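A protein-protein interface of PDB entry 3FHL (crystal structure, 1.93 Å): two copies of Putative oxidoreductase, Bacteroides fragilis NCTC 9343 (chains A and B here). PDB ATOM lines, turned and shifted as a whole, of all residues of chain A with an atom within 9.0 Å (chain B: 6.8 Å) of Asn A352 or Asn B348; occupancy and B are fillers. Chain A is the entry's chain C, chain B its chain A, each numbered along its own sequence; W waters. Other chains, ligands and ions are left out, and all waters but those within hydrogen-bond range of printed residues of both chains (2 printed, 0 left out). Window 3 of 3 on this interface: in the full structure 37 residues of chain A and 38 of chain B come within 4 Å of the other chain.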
ATOM      1  N   PRO A 194      24.650  17.641  -7.186  1.00  0.00           N
ATOM      2  CA  PRO A 194      25.893  17.437  -7.932  1.00  0.00           C
ATOM      3  C   PRO A 194      26.180  18.552  -8.956  1.00  0.00           C
ATOM      4  O   PRO A 194      25.264  19.247  -9.402  1.00  0.00           O
ATOM      5  CB  PRO A 194      25.635  16.111  -8.648  1.00  0.00           C
ATOM      6  CG  PRO A 194      24.185  16.111  -8.893  1.00  0.00           C
ATOM      7  CD  PRO A 194      23.561  16.796  -7.712  1.00  0.00           C
ATOM      8  N   GLU A 195      27.438  18.705  -9.339  1.00  0.00           N
ATOM      9  CA  GLU A 195      27.777  19.580 -10.464  1.00  0.00           C
ATOM     10  C   GLU A 195      27.327  19.004 -11.801  1.00  0.00           C
ATOM     11  O   GLU A 195      26.925  19.748 -12.702  1.00  0.00           O
ATOM     12  CB  GLU A 195      29.279  19.823 -10.509  1.00  0.00           C
ATOM     13  CG  GLU A 195      29.813  20.582  -9.323  1.00  0.00           C
ATOM     14  CD  GLU A 195      31.318  20.698  -9.361  1.00  0.00           C
ATOM     15  OE1 GLU A 195      31.899  20.527 -10.453  1.00  0.00           O
ATOM     16  OE2 GLU A 195      31.921  20.960  -8.301  1.00  0.00           O
ATOM     17  N   ALA A 196      27.394  17.679 -11.935  1.00  0.00           N
ATOM     18  CA  ALA A 196      27.066  17.028 -13.200  1.00  0.00           C
ATOM     19  C   ALA A 196      26.414  15.656 -12.993  1.00  0.00           C
ATOM     20  O   ALA A 196      26.464  15.095 -11.899  1.00  0.00           O
ATOM     21  CB  ALA A 196      28.330  16.914 -14.078  1.00  0.00           C
ATOM     22  N   VAL A 197      25.786  15.136 -14.041  1.00  0.00           N
ATOM     23  CA  VAL A 197      25.127  13.822 -13.984  1.00  0.00           C
ATOM     24  C   VAL A 197      25.535  12.953 -15.184  1.00  0.00           C
ATOM     25  O   VAL A 197      25.494  13.403 -16.326  1.00  0.00           O
ATOM     26  CB  VAL A 197      23.579  13.957 -13.940  1.00  0.00           C
ATOM     27  CG1 VAL A 197      22.877  12.580 -14.117  1.00  0.00           C
ATOM     28  CG2 VAL A 197      23.114  14.612 -12.616  1.00  0.00           C
ATOM     29  N   PHE A 198      25.951  11.716 -14.916  1.00  0.00           N
ATOM     30  CA  PHE A 198      26.010  10.711 -15.956  1.00  0.00           C
ATOM     31  C   PHE A 198      24.939   9.668 -15.663  1.00  0.00           C
ATOM     32  O   PHE A 198      24.747   9.279 -14.511  1.00  0.00           O
ATOM     33  CB  PHE A 198      27.404  10.060 -16.036  1.00  0.00           C
ATOM     34  CG  PHE A 198      27.409   8.746 -16.806  1.00  0.00           C
ATOM     35  CD1 PHE A 198      27.609   8.734 -18.183  1.00  0.00           C
ATOM     36  CD2 PHE A 198      27.170   7.536 -16.158  1.00  0.00           C
ATOM     37  CE1 PHE A 198      27.596   7.530 -18.896  1.00  0.00           C
ATOM     38  CE2 PHE A 198      27.147   6.335 -16.862  1.00  0.00           C
ATOM     39  CZ  PHE A 198      27.365   6.337 -18.236  1.00  0.00           C
ATOM     40  N   HIS A 217      25.523   8.357 -11.955  1.00  0.00           N
ATOM     41  CA  HIS A 217      26.582   8.937 -11.165  1.00  0.00           C
ATOM     42  C   HIS A 217      26.270  10.398 -10.940  1.00  0.00           C
ATOM     43  O   HIS A 217      26.043  11.133 -11.897  1.00  0.00           O
ATOM     44  CB  HIS A 217      27.931   8.782 -11.866  1.00  0.00           C
ATOM     45  CG  HIS A 217      28.339   7.356 -12.022  1.00  0.00           C
ATOM     46  ND1 HIS A 217      28.612   6.551 -10.941  1.00  0.00           N
ATOM     47  CD2 HIS A 217      28.456   6.572 -13.119  1.00  0.00           C
ATOM     48  CE1 HIS A 217      28.908   5.336 -11.365  1.00  0.00           C
ATOM     49  NE2 HIS A 217      28.827   5.325 -12.684  1.00  0.00           N
ATOM     50  N   LEU A 218      26.249  10.794  -9.670  1.00  0.00           N
ATOM     51  CA  LEU A 218      26.071  12.196  -9.296  1.00  0.00           C
ATOM     52  C   LEU A 218      27.466  12.709  -9.020  1.00  0.00           C
ATOM     53  O   LEU A 218      28.126  12.293  -8.056  1.00  0.00           O
ATOM     54  CB  LEU A 218      25.155  12.336  -8.070  1.00  0.00           C
ATOM     55  CG  LEU A 218      23.787  11.675  -8.121  1.00  0.00           C
ATOM     56  CD1 LEU A 218      23.008  12.036  -6.859  1.00  0.00           C
ATOM     57  CD2 LEU A 218      23.033  12.143  -9.336  1.00  0.00           C
ATOM     58  N   LEU A 219      27.933  13.582  -9.904  1.00  0.00           N
ATOM     59  CA  LEU A 219      29.337  13.958  -9.941  1.00  0.00           C
ATOM     60  C   LEU A 219      29.541  15.244  -9.157  1.00  0.00           C
ATOM     61  O   LEU A 219      28.882  16.244  -9.431  1.00  0.00           O
ATOM     62  CB  LEU A 219      29.809  14.110 -11.405  1.00  0.00           C
ATOM     63  CG  LEU A 219      29.475  12.925 -12.340  1.00  0.00           C
ATOM     64  CD1 LEU A 219      29.517  13.293 -13.822  1.00  0.00           C
ATOM     65  CD2 LEU A 219      30.373  11.737 -12.063  1.00  0.00           C
ATOM     66  N   HIS A 220      30.442  15.178  -8.177  1.00  0.00           N
ATOM     67  CA  HIS A 220      30.773  16.277  -7.258  1.00  0.00           C
ATOM     68  C   HIS A 220      29.559  16.897  -6.528  1.00  0.00           C
ATOM     69  O   HIS A 220      29.188  18.049  -6.793  1.00  0.00           O
ATOM     70  CB  HIS A 220      31.611  17.360  -7.964  1.00  0.00           C
ATOM     71  CG  HIS A 220      32.805  16.827  -8.699  1.00  0.00           C
ATOM     72  ND1 HIS A 220      33.937  16.370  -8.056  1.00  0.00           N
ATOM     73  CD2 HIS A 220      33.039  16.676 -10.026  1.00  0.00           C
ATOM     74  CE1 HIS A 220      34.819  15.966  -8.955  1.00  0.00           C
ATOM     75  NE2 HIS A 220      34.297  16.138 -10.156  1.00  0.00           N
ATOM     76  N   ARG A 336      14.762  17.424 -11.217  1.00  0.00           N
ATOM     77  CA  ARG A 336      15.821  18.016 -12.012  1.00  0.00           C
ATOM     78  C   ARG A 336      16.917  16.983 -12.312  1.00  0.00           C
ATOM     79  O   ARG A 336      17.357  16.860 -13.463  1.00  0.00           O
ATOM     80  CB  ARG A 336      16.428  19.220 -11.294  1.00  0.00           C
ATOM     81  CG  ARG A 336      17.516  19.932 -12.081  1.00  0.00           C
ATOM     82  CD  ARG A 336      17.894  21.234 -11.400  1.00  0.00           C
ATOM     83  NE  ARG A 336      18.967  21.950 -12.083  1.00  0.00           N
ATOM     84  CZ  ARG A 336      19.827  22.761 -11.471  1.00  0.00           C
ATOM     85  NH1 ARG A 336      19.747  22.949 -10.157  1.00  0.00           N
ATOM     86  NH2 ARG A 336      20.775  23.375 -12.167  1.00  0.00           N
ATOM     87  N   ILE A 337      17.339  16.250 -11.277  1.00  0.00           N
ATOM     88  CA  ILE A 337      18.297  15.148 -11.434  1.00  0.00           C
ATOM     89  C   ILE A 337      17.776  14.038 -12.359  1.00  0.00           C
ATOM     90  O   ILE A 337      18.513  13.572 -13.233  1.00  0.00           O
ATOM     91  CB  ILE A 337      18.751  14.567 -10.064  1.00  0.00           C
ATOM     92  CG1 ILE A 337      19.299  15.673  -9.159  1.00  0.00           C
ATOM     93  CG2 ILE A 337      19.809  13.458 -10.240  1.00  0.00           C
ATOM     94  CD1 ILE A 337      20.469  16.410  -9.737  1.00  0.00           C
ATOM     95  N   ALA A 340      17.910  15.259 -15.860  1.00  0.00           N
ATOM     96  CA  ALA A 340      19.316  15.244 -16.285  1.00  0.00           C
ATOM     97  C   ALA A 340      19.815  13.840 -16.620  1.00  0.00           C
ATOM     98  O   ALA A 340      20.594  13.669 -17.551  1.00  0.00           O
ATOM     99  CB  ALA A 340      20.197  15.881 -15.253  1.00  0.00           C
ATOM    100  N   ALA A 341      19.350  12.849 -15.864  1.00  0.00           N
ATOM    101  CA  ALA A 341      19.662  11.443 -16.115  1.00  0.00           C
ATOM    102  C   ALA A 341      19.083  10.964 -17.454  1.00  0.00           C
ATOM    103  O   ALA A 341      19.779  10.316 -18.248  1.00  0.00           O
ATOM    104  CB  ALA A 341      19.163  10.569 -14.951  1.00  0.00           C
ATOM    105  N   GLN A 343      18.337  12.963 -19.957  1.00  0.00           N
ATOM    106  CA  GLN A 343      19.020  13.735 -20.992  1.00  0.00           C
ATOM    107  C   GLN A 343      20.417  13.162 -21.290  1.00  0.00           C
ATOM    108  O   GLN A 343      20.824  13.090 -22.442  1.00  0.00           O
ATOM    109  CB  GLN A 343      19.097  15.210 -20.584  1.00  0.00           C
ATOM    110  CG  GLN A 343      19.681  16.138 -21.649  1.00  0.00           C
ATOM    111  CD  GLN A 343      20.065  17.500 -21.103  1.00  0.00           C
ATOM    112  OE1 GLN A 343      19.642  17.895 -20.014  1.00  0.00           O
ATOM    113  NE2 GLN A 343      20.879  18.229 -21.859  1.00  0.00           N
ATOM    114  N   SER A 344      21.135  12.763 -20.245  1.00  0.00           N
ATOM    115  CA  SER A 344      22.450  12.140 -20.367  1.00  0.00           C
ATOM    116  C   SER A 344      22.423  10.855 -21.173  1.00  0.00           C
ATOM    117  O   SER A 344      23.315  10.614 -22.002  1.00  0.00           O
ATOM    118  CB  SER A 344      23.044  11.858 -18.989  1.00  0.00           C
ATOM    119  OG  SER A 344      24.270  11.159 -19.097  1.00  0.00           O
ATOM    120  N   GLU A 347      21.127  11.740 -25.009  1.00  0.00           N
ATOM    121  CA  GLU A 347      22.074  12.537 -25.777  1.00  0.00           C
ATOM    122  C   GLU A 347      23.500  12.005 -25.734  1.00  0.00           C
ATOM    123  O   GLU A 347      24.400  12.601 -26.346  1.00  0.00           O
ATOM    124  CB  GLU A 347      22.049  13.986 -25.294  1.00  0.00           C
ATOM    125  CG  GLU A 347      20.719  14.678 -25.541  1.00  0.00           C
ATOM    126  CD  GLU A 347      20.693  16.138 -25.098  1.00  0.00           C
ATOM    127  OE1 GLU A 347      21.731  16.658 -24.618  1.00  0.00           O
ATOM    128  OE2 GLU A 347      19.614  16.762 -25.230  1.00  0.00           O
ATOM    129  N   LYS A 349      25.722  12.075 -23.358  1.00  0.00           N
ATOM    130  CA  LYS A 349      26.610  13.106 -22.805  1.00  0.00           C
ATOM    131  C   LYS A 349      26.553  13.194 -21.273  1.00  0.00           C
ATOM    132  O   LYS A 349      25.549  12.855 -20.663  1.00  0.00           O
ATOM    133  CB  LYS A 349      26.231  14.475 -23.381  1.00  0.00           C
ATOM    134  CG  LYS A 349      26.677  14.726 -24.825  1.00  0.00           C
ATOM    135  CD  LYS A 349      25.909  15.906 -25.432  1.00  0.00           C
ATOM    136  CE  LYS A 349      26.351  16.212 -26.860  1.00  0.00           C
ATOM    137  NZ  LYS A 349      27.753  16.722 -26.902  1.00  0.00           N
ATOM    138  N   ILE A 350      27.622  13.680 -20.659  1.00  0.00           N
ATOM    139  CA  ILE A 350      27.556  14.132 -19.275  1.00  0.00           C
ATOM    140  C   ILE A 350      26.789  15.461 -19.260  1.00  0.00           C
ATOM    141  O   ILE A 350      27.081  16.361 -20.062  1.00  0.00           O
ATOM    142  CB  ILE A 350      28.962  14.312 -18.693  1.00  0.00           C
ATOM    143  CG1 ILE A 350      29.668  12.948 -18.575  1.00  0.00           C
ATOM    144  CG2 ILE A 350      28.919  15.069 -17.336  1.00  0.00           C
ATOM    145  CD1 ILE A 350      31.074  13.036 -18.008  1.00  0.00           C
ATOM    146  N   VAL A 351      25.805  15.573 -18.366  1.00  0.00           N
ATOM    147  CA  VAL A 351      24.958  16.773 -18.283  1.00  0.00           C
ATOM    148  C   VAL A 351      25.386  17.618 -17.102  1.00  0.00           C
ATOM    149  O   VAL A 351      25.300  17.179 -15.958  1.00  0.00           O
ATOM    150  CB  VAL A 351      23.463  16.416 -18.148  1.00  0.00           C
ATOM    151  CG1 VAL A 351      22.616  17.659 -17.864  1.00  0.00           C
ATOM    152  CG2 VAL A 351      22.966  15.726 -19.395  1.00  0.00           C
ATOM    153  N   ASN A 352      25.850  18.830 -17.388  1.00  0.00           N
ATOM    154  CA  ASN A 352      26.262  19.763 -16.355  1.00  0.00           C
ATOM    155  C   ASN A 352      25.066  20.605 -15.901  1.00  0.00           C
ATOM    156  O   ASN A 352      24.300  21.122 -16.721  1.00  0.00           O
ATOM    157  CB  ASN A 352      27.400  20.659 -16.856  1.00  0.00           C
ATOM    158  CG  ASN A 352      28.638  19.869 -17.249  1.00  0.00           C
ATOM    159  OD1 ASN A 352      29.327  19.298 -16.398  1.00  0.00           O
ATOM    160  ND2 ASN A 352      28.930  19.837 -18.545  1.00  0.00           N
ATOM    161  N   LEU A 353      24.892  20.709 -14.589  1.00  0.00           N
ATOM    162  CA  LEU A 353      23.796  21.488 -14.018  1.00  0.00           C
ATOM    163  C   LEU A 353      24.195  22.962 -13.900  1.00  0.00           C
ATOM    164  O   LEU A 353      25.266  23.276 -13.372  1.00  0.00           O
ATOM    165  CB  LEU A 353      23.412  20.926 -12.643  1.00  0.00           C
ATOM    166  CG  LEU A 353      22.384  19.793 -12.506  1.00  0.00           C
ATOM    167  CD1 LEU A 353      22.750  18.543 -13.260  1.00  0.00           C
ATOM    168  CD2 LEU A 353      22.233  19.452 -11.029  1.00  0.00           C
ATOM    169  N   PHE B 198      32.825   6.184 -20.732  1.00  0.00           N
ATOM    170  CA  PHE B 198      32.735   7.050 -19.547  1.00  0.00           C
ATOM    171  C   PHE B 198      33.706   6.569 -18.474  1.00  0.00           C
ATOM    172  O   PHE B 198      33.759   5.379 -18.161  1.00  0.00           O
ATOM    173  CB  PHE B 198      31.305   7.097 -18.951  1.00  0.00           C
ATOM    174  CG  PHE B 198      31.246   7.780 -17.603  1.00  0.00           C
ATOM    175  CD1 PHE B 198      31.215   9.169 -17.522  1.00  0.00           C
ATOM    176  CD2 PHE B 198      31.292   7.040 -16.421  1.00  0.00           C
ATOM    177  CE1 PHE B 198      31.188   9.811 -16.279  1.00  0.00           C
ATOM    178  CE2 PHE B 198      31.270   7.666 -15.178  1.00  0.00           C
ATOM    179  CZ  PHE B 198      31.213   9.063 -15.109  1.00  0.00           C
ATOM    180  N   ALA B 199      34.453   7.493 -17.884  1.00  0.00           N
ATOM    181  CA  ALA B 199      35.261   7.170 -16.724  1.00  0.00           C
ATOM    182  C   ALA B 199      35.271   8.276 -15.677  1.00  0.00           C
ATOM    183  O   ALA B 199      35.282   9.457 -16.005  1.00  0.00           O
ATOM    184  CB  ALA B 199      36.675   6.867 -17.133  1.00  0.00           C
ATOM    185  N   GLN B 343      40.965  10.643 -20.636  1.00  0.00           N
ATOM    186  CA  GLN B 343      40.413  11.812 -21.328  1.00  0.00           C
ATOM    187  C   GLN B 343      38.999  12.144 -20.835  1.00  0.00           C
ATOM    188  O   GLN B 343      38.657  13.317 -20.668  1.00  0.00           O
ATOM    189  CB  GLN B 343      40.394  11.579 -22.846  1.00  0.00           C
ATOM    190  CG  GLN B 343      39.943  12.780 -23.680  1.00  0.00           C
ATOM    191  CD  GLN B 343      39.646  12.435 -25.132  1.00  0.00           C
ATOM    192  OE1 GLN B 343      40.103  11.419 -25.653  1.00  0.00           O
ATOM    193  NE2 GLN B 343      38.876  13.286 -25.794  1.00  0.00           N
ATOM    194  N   SER B 344      38.184  11.106 -20.630  1.00  0.00           N
ATOM    195  CA  SER B 344      36.815  11.244 -20.106  1.00  0.00           C
ATOM    196  C   SER B 344      36.780  11.932 -18.749  1.00  0.00           C
ATOM    197  O   SER B 344      35.955  12.827 -18.518  1.00  0.00           O
ATOM    198  CB  SER B 344      36.122   9.877 -20.009  1.00  0.00           C
ATOM    199  OG  SER B 344      34.794  10.009 -19.523  1.00  0.00           O
ATOM    200  N   HIS B 345      37.672  11.501 -17.865  1.00  0.00           N
ATOM    201  CA  HIS B 345      37.797  12.070 -16.540  1.00  0.00           C
ATOM    202  C   HIS B 345      38.345  13.505 -16.596  1.00  0.00           C
ATOM    203  O   HIS B 345      37.782  14.414 -15.974  1.00  0.00           O
ATOM    204  CB  HIS B 345      38.676  11.177 -15.669  1.00  0.00           C
ATOM    205  CG  HIS B 345      39.120  11.831 -14.401  1.00  0.00           C
ATOM    206  ND1 HIS B 345      38.248  12.140 -13.379  1.00  0.00           N
ATOM    207  CD2 HIS B 345      40.338  12.263 -14.003  1.00  0.00           C
ATOM    208  CE1 HIS B 345      38.916  12.724 -12.399  1.00  0.00           C
ATOM    209  NE2 HIS B 345      40.185  12.807 -12.751  1.00  0.00           N
ATOM    210  N   ARG B 346      39.426  13.691 -17.355  1.00  0.00           N
ATOM    211  CA  ARG B 346      40.112  14.979 -17.465  1.00  0.00           C
ATOM    212  C   ARG B 346      39.226  16.056 -18.107  1.00  0.00           C
ATOM    213  O   ARG B 346      39.228  17.211 -17.674  1.00  0.00           O
ATOM    214  CB  ARG B 346      41.443  14.794 -18.221  1.00  0.00           C
ATOM    215  CG  ARG B 346      42.080  16.043 -18.832  1.00  0.00           C
ATOM    216  CD  ARG B 346      43.476  15.760 -19.433  1.00  0.00           C
ATOM    217  NE  ARG B 346      43.505  14.623 -20.362  1.00  0.00           N
ATOM    218  CZ  ARG B 346      43.179  14.676 -21.655  1.00  0.00           C
ATOM    219  NH1 ARG B 346      42.784  15.817 -22.215  1.00  0.00           N
ATOM    220  NH2 ARG B 346      43.251  13.578 -22.395  1.00  0.00           N
ATOM    221  N   GLU B 347      38.444  15.665 -19.106  1.00  0.00           N
ATOM    222  CA  GLU B 347      37.603  16.606 -19.844  1.00  0.00           C
ATOM    223  C   GLU B 347      36.136  16.644 -19.403  1.00  0.00           C
ATOM    224  O   GLU B 347      35.351  17.410 -19.961  1.00  0.00           O
ATOM    225  CB  GLU B 347      37.710  16.355 -21.354  1.00  0.00           C
ATOM    226  CG  GLU B 347      39.123  16.606 -21.907  1.00  0.00           C
ATOM    227  CD  GLU B 347      39.261  16.351 -23.405  1.00  0.00           C
ATOM    228  OE1 GLU B 347      38.250  16.036 -24.079  1.00  0.00           O
ATOM    229  OE2 GLU B 347      40.404  16.464 -23.905  1.00  0.00           O
ATOM    230  N   ASN B 348      35.777  15.820 -18.414  1.00  0.00           N
ATOM    231  CA  ASN B 348      34.391  15.713 -17.925  1.00  0.00           C
ATOM    232  C   ASN B 348      33.407  15.451 -19.077  1.00  0.00           C
ATOM    233  O   ASN B 348      32.356  16.099 -19.204  1.00  0.00           O
ATOM    234  CB  ASN B 348      34.026  16.938 -17.049  1.00  0.00           C
ATOM    235  CG  ASN B 348      32.632  16.848 -16.430  1.00  0.00           C
ATOM    236  OD1 ASN B 348      32.229  15.810 -15.895  1.00  0.00           O
ATOM    237  ND2 ASN B 348      31.883  17.946 -16.513  1.00  0.00           N
ATOM    238  N   LYS B 349      33.767  14.498 -19.941  1.00  0.00           N
ATOM    239  CA  LYS B 349      32.962  14.181 -21.125  1.00  0.00           C
ATOM    240  C   LYS B 349      32.901  12.677 -21.373  1.00  0.00           C
ATOM    241  O   LYS B 349      33.810  11.964 -20.992  1.00  0.00           O
ATOM    242  CB  LYS B 349      33.553  14.864 -22.366  1.00  0.00           C
ATOM    243  CG  LYS B 349      33.283  16.367 -22.478  1.00  0.00           C
ATOM    244  CD  LYS B 349      34.094  16.989 -23.617  1.00  0.00           C
ATOM    245  CE  LYS B 349      34.021  18.516 -23.622  1.00  0.00           C
ATOM    246  NZ  LYS B 349      32.740  19.012 -24.207  1.00  0.00           N
ATOM    247  N   ILE B 350      31.830  12.200 -22.004  1.00  0.00           N
ATOM    248  CA  ILE B 350      31.840  10.874 -22.617  1.00  0.00           C
ATOM    249  C   ILE B 350      32.780  10.954 -23.842  1.00  0.00           C
ATOM    250  O   ILE B 350      32.668  11.879 -24.650  1.00  0.00           O
ATOM    251  CB  ILE B 350      30.409  10.424 -22.995  1.00  0.00           C
ATOM    252  CG1 ILE B 350      29.587  10.167 -21.706  1.00  0.00           C
ATOM    253  CG2 ILE B 350      30.428   9.201 -23.911  1.00  0.00           C
ATOM    254  CD1 ILE B 350      28.147   9.734 -21.929  1.00  0.00           C
HETATM  255  O   HOH W   1      30.855  18.176 -20.032  1.00  0.00           O
HETATM  256  O   HOH W   2      29.863  14.484 -22.509  1.00  0.00           O
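The side-chain amide nitrogen (ND2) of Asn B348 is in hydrogen-bond range of the side-chain amide oxygen (OD1) of Asn A352.
The side-chain hydroxyl (OG) of Ser B344 sits at hydrogen-bond distance from the backbone carbonyl oxygen (O) of Lys B349.
The backbone carbonyl oxygen (O) of Phe A198 lies within hydrogen-bond range of the backbone NH (N) of His A217 (2.8 Å).
The backbone carbonyl oxygen of Lys A349 is in hydrogen-bond range of the side-chain hydroxyl of Ser A344 (2.6 Å).
Among the printed residues, merely in contact across the chains: Phe A198 with Phe B198 (3.7 Å), Phe A198 with Ile B350 (3.8 Å), His A217 with Phe B198 (3.7 Å), Lys A349 with Ile B350 (3.7 Å), Ile A350 with Phe B198 (3.7 Å), Ile A350 with Asn B348 (3.5 Å) and Ile A350 with Lys B349 (3.6 Å).
Leu A218 touches none of the printed residues of chain B.
Printed residues of chain B within 4 Å of Lys A349: Ile B350 (3.7 Å).
Printed residues of chain B within 4 Å of Ile A350: Phe B198 (3.7 Å), Asn B348 (3.5 Å) and Lys B349 (3.6 Å).
Of chain B, only Asn B348 (2.9 Å) comes within 4 Å of Asn A352.
Gln B343 touches none of the printed residues of chain A.
Of the printed residues of chain A, Lys B349 touches Ile A350 (3.6 Å).
The nearest printed residue of chain B that does not touch Asn A352 is Lys B349 (6.8 Å).
Of the 10 printed residues of chain B, 4 touch a printed residue of chain A.
Printed residues of chain B that touch a printed residue of chain A: Phe B198, Asn B348, Lys B349 and Ile B350.
Hydrophobic or aromatic side chains of chain B within 4 Å of the printed part of chain A: Phe B198 and Ile B350.
Of the 21 printed residues of chain A, 5 touch a printed residue of chain B.
Hydrophobic or aromatic side chains of chain A that line the printed part of chain B: Phe A198, His A217 and Ile A350.
Phe B198 touches its own counterpart, Phe A198.
Phe A198 touches Ile B350, and with the chains exchanged Ile A350 touches Phe B198.
Lys A349 touches Ile B350, and with the chains exchanged Ile A350 touches Lys B349.
Positions printed for both chains: 198, 343, 344, 347, 349 and 350.
Water W1 lies within hydrogen-bond range of the backbone carbonyl oxygen of Asn B348 and the side-chain amide nitrogen of Asn A352.
Water W2 bridges the backbone NH of Ile A350 and the backbone NH of Ile B350.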
